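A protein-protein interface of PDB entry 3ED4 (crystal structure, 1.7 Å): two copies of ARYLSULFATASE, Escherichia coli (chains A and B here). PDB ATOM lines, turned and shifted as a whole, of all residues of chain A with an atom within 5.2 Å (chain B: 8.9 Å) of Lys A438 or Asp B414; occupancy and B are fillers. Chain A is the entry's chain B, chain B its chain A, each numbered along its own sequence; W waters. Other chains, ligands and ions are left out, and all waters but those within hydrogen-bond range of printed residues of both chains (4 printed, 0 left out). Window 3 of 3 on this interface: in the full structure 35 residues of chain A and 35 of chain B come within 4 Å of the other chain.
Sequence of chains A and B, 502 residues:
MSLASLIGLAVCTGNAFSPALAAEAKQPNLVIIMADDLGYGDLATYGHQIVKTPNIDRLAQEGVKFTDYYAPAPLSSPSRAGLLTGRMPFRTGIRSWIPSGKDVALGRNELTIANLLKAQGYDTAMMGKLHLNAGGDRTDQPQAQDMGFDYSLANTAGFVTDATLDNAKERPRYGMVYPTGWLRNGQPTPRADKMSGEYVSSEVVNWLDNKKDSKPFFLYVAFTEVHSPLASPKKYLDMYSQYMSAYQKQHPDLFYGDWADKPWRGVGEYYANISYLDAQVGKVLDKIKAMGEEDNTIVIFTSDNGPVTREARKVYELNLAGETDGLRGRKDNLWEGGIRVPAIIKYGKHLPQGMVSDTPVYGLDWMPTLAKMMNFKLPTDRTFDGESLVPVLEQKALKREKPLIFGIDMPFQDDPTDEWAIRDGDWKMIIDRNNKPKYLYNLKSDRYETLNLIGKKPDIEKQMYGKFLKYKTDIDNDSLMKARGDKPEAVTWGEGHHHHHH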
ATOM      1  N   ARG A 328      29.545  38.591 -10.664  1.00  0.00           N
ATOM      2  CA  ARG A 328      30.009  37.941  -9.433  1.00  0.00           C
ATOM      3  C   ARG A 328      31.528  38.073  -9.191  1.00  0.00           C
ATOM      4  O   ARG A 328      32.329  37.944 -10.115  1.00  0.00           O
ATOM      5  CB  ARG A 328      29.606  36.455  -9.431  1.00  0.00           C
ATOM      6  CG  ARG A 328      29.780  35.796  -8.062  1.00  0.00           C
ATOM      7  CD  ARG A 328      29.142  34.413  -7.945  1.00  0.00           C
ATOM      8  NE  ARG A 328      29.266  33.925  -6.572  1.00  0.00           N
ATOM      9  CZ  ARG A 328      28.819  32.753  -6.118  1.00  0.00           C
ATOM     10  NH1 ARG A 328      28.188  31.897  -6.927  1.00  0.00           N
ATOM     11  NH2 ARG A 328      29.009  32.437  -4.841  1.00  0.00           N
ATOM     12  N   TRP A 335      35.380  34.117 -10.842  1.00  0.00           N
ATOM     13  CA  TRP A 335      34.069  34.563 -11.306  1.00  0.00           C
ATOM     14  C   TRP A 335      34.213  35.805 -12.220  1.00  0.00           C
ATOM     15  O   TRP A 335      35.275  36.464 -12.241  1.00  0.00           O
ATOM     16  CB  TRP A 335      33.131  34.864 -10.135  1.00  0.00           C
ATOM     17  CG  TRP A 335      32.651  33.663  -9.344  1.00  0.00           C
ATOM     18  CD1 TRP A 335      31.952  32.583  -9.821  1.00  0.00           C
ATOM     19  CD2 TRP A 335      32.784  33.467  -7.936  1.00  0.00           C
ATOM     20  NE1 TRP A 335      31.659  31.716  -8.790  1.00  0.00           N
ATOM     21  CE2 TRP A 335      32.162  32.232  -7.622  1.00  0.00           C
ATOM     22  CE3 TRP A 335      33.381  34.210  -6.900  1.00  0.00           C
ATOM     23  CZ2 TRP A 335      32.124  31.721  -6.315  1.00  0.00           C
ATOM     24  CZ3 TRP A 335      33.337  33.698  -5.592  1.00  0.00           C
ATOM     25  CH2 TRP A 335      32.710  32.468  -5.317  1.00  0.00           C
ATOM     26  N   ASP A 418      39.763  29.841  -5.978  1.00  0.00           N
ATOM     27  CA  ASP A 418      39.887  28.731  -6.921  1.00  0.00           C
ATOM     28  C   ASP A 418      41.103  28.984  -7.803  1.00  0.00           C
ATOM     29  O   ASP A 418      41.630  30.101  -7.830  1.00  0.00           O
ATOM     30  CB  ASP A 418      38.605  28.572  -7.737  1.00  0.00           C
ATOM     31  CG  ASP A 418      37.399  28.258  -6.867  1.00  0.00           C
ATOM     32  OD1 ASP A 418      37.379  27.176  -6.249  1.00  0.00           O
ATOM     33  OD2 ASP A 418      36.472  29.099  -6.797  1.00  0.00           O
ATOM     34  N   ILE A 430      34.893  26.326 -13.354  1.00  0.00           N
ATOM     35  CA  ILE A 430      35.905  26.813 -12.420  1.00  0.00           C
ATOM     36  C   ILE A 430      36.434  25.627 -11.608  1.00  0.00           C
ATOM     37  O   ILE A 430      35.657  24.861 -11.041  1.00  0.00           O
ATOM     38  CB  ILE A 430      35.334  27.911 -11.485  1.00  0.00           C
ATOM     39  CG1 ILE A 430      34.851  29.122 -12.315  1.00  0.00           C
ATOM     40  CG2 ILE A 430      36.368  28.307 -10.442  1.00  0.00           C
ATOM     41  CD1 ILE A 430      34.245  30.294 -11.493  1.00  0.00           C
ATOM     42  N   ILE A 431      37.759  25.504 -11.569  1.00  0.00           N
ATOM     43  CA  ILE A 431      38.467  24.396 -10.925  1.00  0.00           C
ATOM     44  C   ILE A 431      39.058  24.877  -9.596  1.00  0.00           C
ATOM     45  O   ILE A 431      39.757  25.902  -9.568  1.00  0.00           O
ATOM     46  CB  ILE A 431      39.625  23.877 -11.841  1.00  0.00           C
ATOM     47  CG1 ILE A 431      39.133  23.521 -13.255  1.00  0.00           C
ATOM     48  CG2 ILE A 431      40.360  22.714 -11.210  1.00  0.00           C
ATOM     49  CD1 ILE A 431      37.986  22.534 -13.307  1.00  0.00           C
ATOM     50  N   ASP A 432      38.780  24.151  -8.505  1.00  0.00           N
ATOM     51  CA  ASP A 432      39.352  24.494  -7.191  1.00  0.00           C
ATOM     52  C   ASP A 432      40.859  24.174  -7.067  1.00  0.00           C
ATOM     53  O   ASP A 432      41.470  23.634  -7.996  1.00  0.00           O
ATOM     54  CB  ASP A 432      38.526  23.885  -6.034  1.00  0.00           C
ATOM     55  CG  ASP A 432      38.673  22.362  -5.919  1.00  0.00           C
ATOM     56  OD1 ASP A 432      39.682  21.798  -6.393  1.00  0.00           O
ATOM     57  OD2 ASP A 432      37.778  21.724  -5.322  1.00  0.00           O
ATOM     58  N   LYS A 436      39.813  19.857  -8.624  1.00  0.00           N
ATOM     59  CA  LYS A 436      38.446  19.364  -8.793  1.00  0.00           C
ATOM     60  C   LYS A 436      37.510  20.453  -9.328  1.00  0.00           C
ATOM     61  O   LYS A 436      37.612  21.611  -8.909  1.00  0.00           O
ATOM     62  CB  LYS A 436      37.902  18.831  -7.462  1.00  0.00           C
ATOM     63  CG  LYS A 436      38.758  17.765  -6.814  1.00  0.00           C
ATOM     64  CD  LYS A 436      38.083  17.170  -5.584  1.00  0.00           C
ATOM     65  CE  LYS A 436      38.946  16.081  -4.957  1.00  0.00           C
ATOM     66  NZ  LYS A 436      39.197  14.947  -5.899  1.00  0.00           N
ATOM     67  N   PRO A 437      36.592  20.085 -10.247  1.00  0.00           N
ATOM     68  CA  PRO A 437      35.581  21.053 -10.673  1.00  0.00           C
ATOM     69  C   PRO A 437      34.761  21.498  -9.466  1.00  0.00           C
ATOM     70  O   PRO A 437      34.419  20.678  -8.609  1.00  0.00           O
ATOM     71  CB  PRO A 437      34.706  20.260 -11.644  1.00  0.00           C
ATOM     72  CG  PRO A 437      35.511  19.076 -12.041  1.00  0.00           C
ATOM     73  CD  PRO A 437      36.430  18.776 -10.910  1.00  0.00           C
ATOM     74  N   LYS A 438      34.506  22.798  -9.365  1.00  0.00           N
ATOM     75  CA  LYS A 438      33.728  23.305  -8.252  1.00  0.00           C
ATOM     76  C   LYS A 438      32.465  23.985  -8.741  1.00  0.00           C
ATOM     77  O   LYS A 438      31.438  23.894  -8.082  1.00  0.00           O
ATOM     78  CB  LYS A 438      34.548  24.249  -7.360  1.00  0.00           C
ATOM     79  CG  LYS A 438      33.922  24.421  -5.975  1.00  0.00           C
ATOM     80  CD  LYS A 438      34.566  25.518  -5.164  1.00  0.00           C
ATOM     81  CE  LYS A 438      33.806  25.708  -3.866  1.00  0.00           C
ATOM     82  NZ  LYS A 438      34.430  26.765  -3.018  1.00  0.00           N
ATOM     83  N   TYR A 439      32.560  24.665  -9.887  1.00  0.00           N
ATOM     84  CA  TYR A 439      31.437  25.370 -10.495  1.00  0.00           C
ATOM     85  C   TYR A 439      31.364  25.116 -11.993  1.00  0.00           C
ATOM     86  O   TYR A 439      32.393  25.027 -12.672  1.00  0.00           O
ATOM     87  CB  TYR A 439      31.542  26.889 -10.275  1.00  0.00           C
ATOM     88  CG  TYR A 439      31.799  27.340  -8.847  1.00  0.00           C
ATOM     89  CD1 TYR A 439      30.820  27.206  -7.854  1.00  0.00           C
ATOM     90  CD2 TYR A 439      33.016  27.929  -8.495  1.00  0.00           C
ATOM     91  CE1 TYR A 439      31.059  27.630  -6.533  1.00  0.00           C
ATOM     92  CE2 TYR A 439      33.261  28.351  -7.185  1.00  0.00           C
ATOM     93  CZ  TYR A 439      32.282  28.199  -6.211  1.00  0.00           C
ATOM     94  OH  TYR A 439      32.530  28.620  -4.918  1.00  0.00           O
ATOM     95  N   LEU A 440      30.136  25.016 -12.490  1.00  0.00           N
ATOM     96  CA  LEU A 440      29.852  24.999 -13.917  1.00  0.00           C
ATOM     97  C   LEU A 440      28.667  25.914 -14.169  1.00  0.00           C
ATOM     98  O   LEU A 440      27.608  25.753 -13.552  1.00  0.00           O
ATOM     99  CB  LEU A 440      29.561  23.577 -14.420  1.00  0.00           C
ATOM    100  CG  LEU A 440      29.162  23.449 -15.897  1.00  0.00           C
ATOM    101  CD1 LEU A 440      30.350  23.755 -16.826  1.00  0.00           C
ATOM    102  CD2 LEU A 440      28.570  22.071 -16.194  1.00  0.00           C
ATOM    103  N   TYR A 441      28.857  26.880 -15.063  1.00  0.00           N
ATOM    104  CA  TYR A 441      27.817  27.831 -15.407  1.00  0.00           C
ATOM    105  C   TYR A 441      27.604  27.923 -16.911  1.00  0.00           C
ATOM    106  O   TYR A 441      28.551  27.802 -17.692  1.00  0.00           O
ATOM    107  CB  TYR A 441      28.163  29.245 -14.879  1.00  0.00           C
ATOM    108  CG  TYR A 441      28.502  29.331 -13.405  1.00  0.00           C
ATOM    109  CD1 TYR A 441      27.527  29.108 -12.424  1.00  0.00           C
ATOM    110  CD2 TYR A 441      29.793  29.671 -12.991  1.00  0.00           C
ATOM    111  CE1 TYR A 441      27.836  29.212 -11.061  1.00  0.00           C
ATOM    112  CE2 TYR A 441      30.114  29.777 -11.642  1.00  0.00           C
ATOM    113  CZ  TYR A 441      29.133  29.542 -10.684  1.00  0.00           C
ATOM    114  OH  TYR A 441      29.434  29.637  -9.347  1.00  0.00           O
ATOM    115  N   ASN A 452      24.821  27.038 -10.268  1.00  0.00           N
ATOM    116  CA  ASN A 452      25.832  26.017 -10.461  1.00  0.00           C
ATOM    117  C   ASN A 452      25.211  24.721 -10.998  1.00  0.00           C
ATOM    118  O   ASN A 452      24.232  24.216 -10.446  1.00  0.00           O
ATOM    119  CB  ASN A 452      26.558  25.769  -9.139  1.00  0.00           C
ATOM    120  CG  ASN A 452      27.800  24.914  -9.296  1.00  0.00           C
ATOM    121  OD1 ASN A 452      28.153  24.486 -10.398  1.00  0.00           O
ATOM    122  ND2 ASN A 452      28.477  24.666  -8.183  1.00  0.00           N
ATOM    123  N   ILE A 454      27.027  21.830 -11.752  1.00  0.00           N
ATOM    124  CA  ILE A 454      27.786  20.634 -11.369  1.00  0.00           C
ATOM    125  C   ILE A 454      26.807  19.582 -10.842  1.00  0.00           C
ATOM    126  O   ILE A 454      25.975  19.876  -9.975  1.00  0.00           O
ATOM    127  CB  ILE A 454      28.891  20.944 -10.308  1.00  0.00           C
ATOM    128  CG1 ILE A 454      30.029  21.779 -10.916  1.00  0.00           C
ATOM    129  CG2 ILE A 454      29.435  19.656  -9.649  1.00  0.00           C
ATOM    130  CD1 ILE A 454      30.911  21.065 -11.937  1.00  0.00           C
ATOM    131  N   TRP B  97      18.045  28.868   8.302  1.00  0.00           N
ATOM    132  CA  TRP B  97      16.833  28.769   7.482  1.00  0.00           C
ATOM    133  C   TRP B  97      15.837  27.735   8.031  1.00  0.00           C
ATOM    134  O   TRP B  97      16.228  26.753   8.665  1.00  0.00           O
ATOM    135  CB  TRP B  97      17.204  28.437   6.017  1.00  0.00           C
ATOM    136  CG  TRP B  97      18.269  27.355   5.852  1.00  0.00           C
ATOM    137  CD1 TRP B  97      18.268  26.106   6.414  1.00  0.00           C
ATOM    138  CD2 TRP B  97      19.469  27.429   5.063  1.00  0.00           C
ATOM    139  NE1 TRP B  97      19.389  25.409   6.040  1.00  0.00           N
ATOM    140  CE2 TRP B  97      20.143  26.191   5.207  1.00  0.00           C
ATOM    141  CE3 TRP B  97      20.038  28.419   4.249  1.00  0.00           C
ATOM    142  CZ2 TRP B  97      21.363  25.916   4.569  1.00  0.00           C
ATOM    143  CZ3 TRP B  97      21.252  28.142   3.611  1.00  0.00           C
ATOM    144  CH2 TRP B  97      21.898  26.899   3.779  1.00  0.00           C
ATOM    145  N   ALA B 312      25.980  39.235  -4.774  1.00  0.00           N
ATOM    146  CA  ALA B 312      24.914  38.228  -4.881  1.00  0.00           C
ATOM    147  C   ALA B 312      25.481  36.811  -4.901  1.00  0.00           C
ATOM    148  O   ALA B 312      26.436  36.519  -5.632  1.00  0.00           O
ATOM    149  CB  ALA B 312      24.034  38.473  -6.104  1.00  0.00           C
ATOM    150  N   ARG B 313      24.867  35.945  -4.097  1.00  0.00           N
ATOM    151  CA  ARG B 313      25.297  34.557  -3.917  1.00  0.00           C
ATOM    152  C   ARG B 313      24.231  33.577  -4.430  1.00  0.00           C
ATOM    153  O   ARG B 313      24.485  32.385  -4.547  1.00  0.00           O
ATOM    154  CB  ARG B 313      25.538  34.266  -2.433  1.00  0.00           C
ATOM    155  CG  ARG B 313      26.812  34.905  -1.890  1.00  0.00           C
ATOM    156  CD  ARG B 313      26.933  34.849  -0.377  1.00  0.00           C
ATOM    157  NE  ARG B 313      28.097  35.633   0.049  1.00  0.00           N
ATOM    158  CZ  ARG B 313      28.304  36.105   1.277  1.00  0.00           C
ATOM    159  NH1 ARG B 313      27.430  35.879   2.260  1.00  0.00           N
ATOM    160  NH2 ARG B 313      29.402  36.809   1.518  1.00  0.00           N
ATOM    161  N   LYS B 314      23.038  34.100  -4.695  1.00  0.00           N
ATOM    162  CA  LYS B 314      21.863  33.303  -5.071  1.00  0.00           C
ATOM    163  C   LYS B 314      21.095  34.039  -6.158  1.00  0.00           C
ATOM    164  O   LYS B 314      21.179  35.269  -6.272  1.00  0.00           O
ATOM    165  CB  LYS B 314      20.934  33.113  -3.869  1.00  0.00           C
ATOM    166  CG  LYS B 314      21.595  32.636  -2.568  1.00  0.00           C
ATOM    167  CD  LYS B 314      21.953  31.156  -2.624  1.00  0.00           C
ATOM    168  CE  LYS B 314      23.095  30.793  -1.665  1.00  0.00           C
ATOM    169  NZ  LYS B 314      22.776  30.996  -0.217  1.00  0.00           N
ATOM    170  N   ASP B 332      24.437  36.491   6.060  1.00  0.00           N
ATOM    171  CA  ASP B 332      25.050  35.138   6.179  1.00  0.00           C
ATOM    172  C   ASP B 332      26.301  35.140   7.064  1.00  0.00           C
ATOM    173  O   ASP B 332      26.602  34.140   7.712  1.00  0.00           O
ATOM    174  CB  ASP B 332      25.433  34.455   4.840  1.00  0.00           C
ATOM    175  CG  ASP B 332      24.300  34.435   3.808  1.00  0.00           C
ATOM    176  OD1 ASP B 332      23.123  34.613   4.178  1.00  0.00           O
ATOM    177  OD2 ASP B 332      24.623  34.284   2.615  1.00  0.00           O
ATOM    178  N   MET B 410      25.015  27.279   8.764  1.00  0.00           N
ATOM    179  CA  MET B 410      24.684  27.400   7.345  1.00  0.00           C
ATOM    180  C   MET B 410      25.662  26.572   6.513  1.00  0.00           C
ATOM    181  O   MET B 410      26.691  27.074   6.069  1.00  0.00           O
ATOM    182  CB  MET B 410      24.683  28.883   6.914  1.00  0.00           C
ATOM    183  CG  MET B 410      24.130  29.148   5.505  1.00  0.00           C
ATOM    184  SD  MET B 410      24.188  30.870   4.942  1.00  0.00           S
ATOM    185  CE  MET B 410      23.607  31.615   6.392  1.00  0.00           C
ATOM    186  N   PRO B 411      25.351  25.276   6.318  1.00  0.00           N
ATOM    187  CA  PRO B 411      26.217  24.417   5.508  1.00  0.00           C
ATOM    188  C   PRO B 411      26.099  24.675   3.995  1.00  0.00           C
ATOM    189  O   PRO B 411      25.217  25.430   3.549  1.00  0.00           O
ATOM    190  CB  PRO B 411      25.735  22.997   5.871  1.00  0.00           C
ATOM    191  CG  PRO B 411      24.313  23.175   6.261  1.00  0.00           C
ATOM    192  CD  PRO B 411      24.191  24.547   6.865  1.00  0.00           C
ATOM    193  N   PHE B 412      27.011  24.060   3.239  1.00  0.00           N
ATOM    194  CA  PHE B 412      26.970  23.964   1.758  1.00  0.00           C
ATOM    195  C   PHE B 412      27.085  25.296   1.004  1.00  0.00           C
ATOM    196  O   PHE B 412      26.563  25.425  -0.103  1.00  0.00           O
ATOM    197  CB  PHE B 412      25.722  23.191   1.262  1.00  0.00           C
ATOM    198  CG  PHE B 412      25.316  22.036   2.141  1.00  0.00           C
ATOM    199  CD1 PHE B 412      26.188  20.977   2.386  1.00  0.00           C
ATOM    200  CD2 PHE B 412      24.050  22.013   2.717  1.00  0.00           C
ATOM    201  CE1 PHE B 412      25.804  19.915   3.204  1.00  0.00           C
ATOM    202  CE2 PHE B 412      23.656  20.954   3.530  1.00  0.00           C
ATOM    203  CZ  PHE B 412      24.541  19.906   3.774  1.00  0.00           C
ATOM    204  N   GLN B 413      27.749  26.287   1.596  1.00  0.00           N
ATOM    205  CA  GLN B 413      27.903  27.575   0.915  1.00  0.00           C
ATOM    206  C   GLN B 413      29.136  27.532   0.031  1.00  0.00           C
ATOM    207  O   GLN B 413      30.093  26.799   0.330  1.00  0.00           O
ATOM    208  CB  GLN B 413      27.954  28.731   1.917  1.00  0.00           C
ATOM    209  CG  GLN B 413      26.677  28.903   2.760  1.00  0.00           C
ATOM    210  CD  GLN B 413      25.396  28.878   1.931  1.00  0.00           C
ATOM    211  OE1 GLN B 413      25.063  29.847   1.242  1.00  0.00           O
ATOM    212  NE2 GLN B 413      24.663  27.765   2.008  1.00  0.00           N
ATOM    213  N   ASP B 414      29.100  28.278  -1.075  1.00  0.00           N
ATOM    214  CA  ASP B 414      30.235  28.348  -2.008  1.00  0.00           C
ATOM    215  C   ASP B 414      31.508  28.739  -1.265  1.00  0.00           C
ATOM    216  O   ASP B 414      32.527  28.059  -1.367  1.00  0.00           O
ATOM    217  CB  ASP B 414      29.956  29.342  -3.137  1.00  0.00           C
ATOM    218  CG  ASP B 414      28.875  28.868  -4.088  1.00  0.00           C
ATOM    219  OD1 ASP B 414      28.604  27.646  -4.160  1.00  0.00           O
ATOM    220  OD2 ASP B 414      28.303  29.733  -4.776  1.00  0.00           O
ATOM    221  N   ASP B 415      31.432  29.836  -0.511  1.00  0.00           N
ATOM    222  CA  ASP B 415      32.454  30.159   0.474  1.00  0.00           C
ATOM    223  C   ASP B 415      31.892  29.752   1.833  1.00  0.00           C
ATOM    224  O   ASP B 415      30.923  30.353   2.303  1.00  0.00           O
ATOM    225  CB  ASP B 415      32.802  31.647   0.441  1.00  0.00           C
ATOM    226  CG  ASP B 415      33.479  32.059  -0.849  1.00  0.00           C
ATOM    227  OD1 ASP B 415      34.455  31.393  -1.253  1.00  0.00           O
ATOM    228  OD2 ASP B 415      33.051  33.066  -1.451  1.00  0.00           O
ATOM    229  N   PRO B 416      32.466  28.697   2.443  1.00  0.00           N
ATOM    230  CA  PRO B 416      31.942  28.172   3.712  1.00  0.00           C
ATOM    231  C   PRO B 416      31.785  29.242   4.797  1.00  0.00           C
ATOM    232  O   PRO B 416      32.702  30.035   5.052  1.00  0.00           O
ATOM    233  CB  PRO B 416      32.983  27.118   4.110  1.00  0.00           C
ATOM    234  CG  PRO B 416      33.548  26.661   2.804  1.00  0.00           C
ATOM    235  CD  PRO B 416      33.630  27.919   1.972  1.00  0.00           C
ATOM    236  N   THR B 417      30.596  29.292   5.388  1.00  0.00           N
ATOM    237  CA  THR B 417      30.319  30.213   6.475  1.00  0.00           C
ATOM    238  C   THR B 417      31.013  29.731   7.745  1.00  0.00           C
ATOM    239  O   THR B 417      31.371  28.554   7.862  1.00  0.00           O
ATOM    240  CB  THR B 417      28.811  30.317   6.747  1.00  0.00           C
ATOM    241  OG1 THR B 417      28.289  29.015   7.054  1.00  0.00           O
ATOM    242  CG2 THR B 417      28.085  30.900   5.542  1.00  0.00           C
HETATM  243  O   HOH W   1      27.651  28.959  -7.584  1.00  0.00           O
HETATM  244  O   HOH W   2      30.504  33.224  -2.452  1.00  0.00           O
HETATM  245  O   HOH W   3      29.203  36.312  -4.764  1.00  0.00           O
HETATM  246  O   HOH W   4      27.071  26.057  -5.683  1.00  0.00           O
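The side-chain carboxylate of Asp B414 is in salt-bridge range of the guanidinium group of Arg A328 (2.8 Å).
The backbone carbonyl oxygen (O) of Asp B414 sits at hydrogen-bond distance from the side-chain amino group (NZ) of Lys A438 (2.8 Å).
OH of Tyr A441 sits at hydrogen-bond distance from NE1 of Trp A335 (3.1 Å).
The backbone carbonyl oxygen (O) of Ile A430 is in hydrogen-bond range of the backbone NH (N) of Lys A438, 2.9 Å away.
The backbone carbonyl oxygen (O) of Tyr A439 lies within hydrogen-bond range of the backbone NH (N) of Ile A430 (2.9 Å).
NZ of Lys A438 is in hydrogen-bond range of OH of Tyr A439 (3.3 Å).
The backbone carbonyl oxygen (O) of Lys A438 is in hydrogen-bond range of the side-chain amide nitrogen (ND2) of Asn A452.
Among the printed residues, pairs that only touch across the chains: Arg A328 with Ala B312 (3.95 Å), Trp A335 with Asp B415 (3.9 Å) and Tyr A439 with Asp B414 (3.2 Å).
Lys A438 touches just one residue of chain B: Asp B414 (2.8 Å).
Asp B414 touches just these residues of chain A: Arg A328, Lys A438 and Tyr A439.
No residue of chain B comes within 4 Å of Pro A437.
Tyr A439 touches just one residue of chain B: Asp B414 (3.2 Å).
Of the printed residues of chain B, Arg A328 touches Ala B312 and Asp B414.
Of the printed residues of chain A, Asp B415 touches Trp A335.
Of the printed residues of chain A, Ala B312 touches Arg A328 (3.95 Å).
Printed residues of chain B within 4 Å of Trp A335: Asp B415 (3.9 Å).
Asp A418 touches none of the printed residues of chain B.
Arg B313 touches none of the printed residues of chain A.
The nearest residue of chain B that does not touch Lys A438 is Asp B415 (5.0 Å).
The nearest residue of chain A that does not touch Asp B414 is Trp A335 (4.5 Å).
The nearest printed residue of chain B that does not touch Trp A335 is Asp B414 (4.5 Å).
Hydrophobic or aromatic side chains of chain A within 4 Å of the printed part of chain B: Trp A335 and Tyr A439.
Of the 13 printed residues of chain B, 3 touch a printed residue of chain A.
Along chain B the printed residues that touch a printed residue of chain A span positions 312 to 415.
Among the printed residues, Asp or Glu carboxylates within 4 Å of a Lys or Arg side-chain nitrogen of the other chain: Arg A328 with Asp B414 (2.8 Å).
No position is printed for both chains.
Of the 5 pairs that touch across the chains among the printed residues, none has its exchanged pair printed and touching as well.
Water W1 lies within hydrogen-bond range of OH of Tyr A441 (2.6 Å), OD2 of Asp B414 (3.0 Å) and NH1 of Arg A328 (3.1 Å).
Water W4 lies within hydrogen-bond range of OD1 of Asp B414 and ND2 of Asn A452.
Water W2 lies within hydrogen-bond range of the side-chain carboxylate of Asp B415 and the guanidinium group of Arg A328.
Water W3 lies within hydrogen-bond range of O of Ala B312 and NE of Arg A328.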
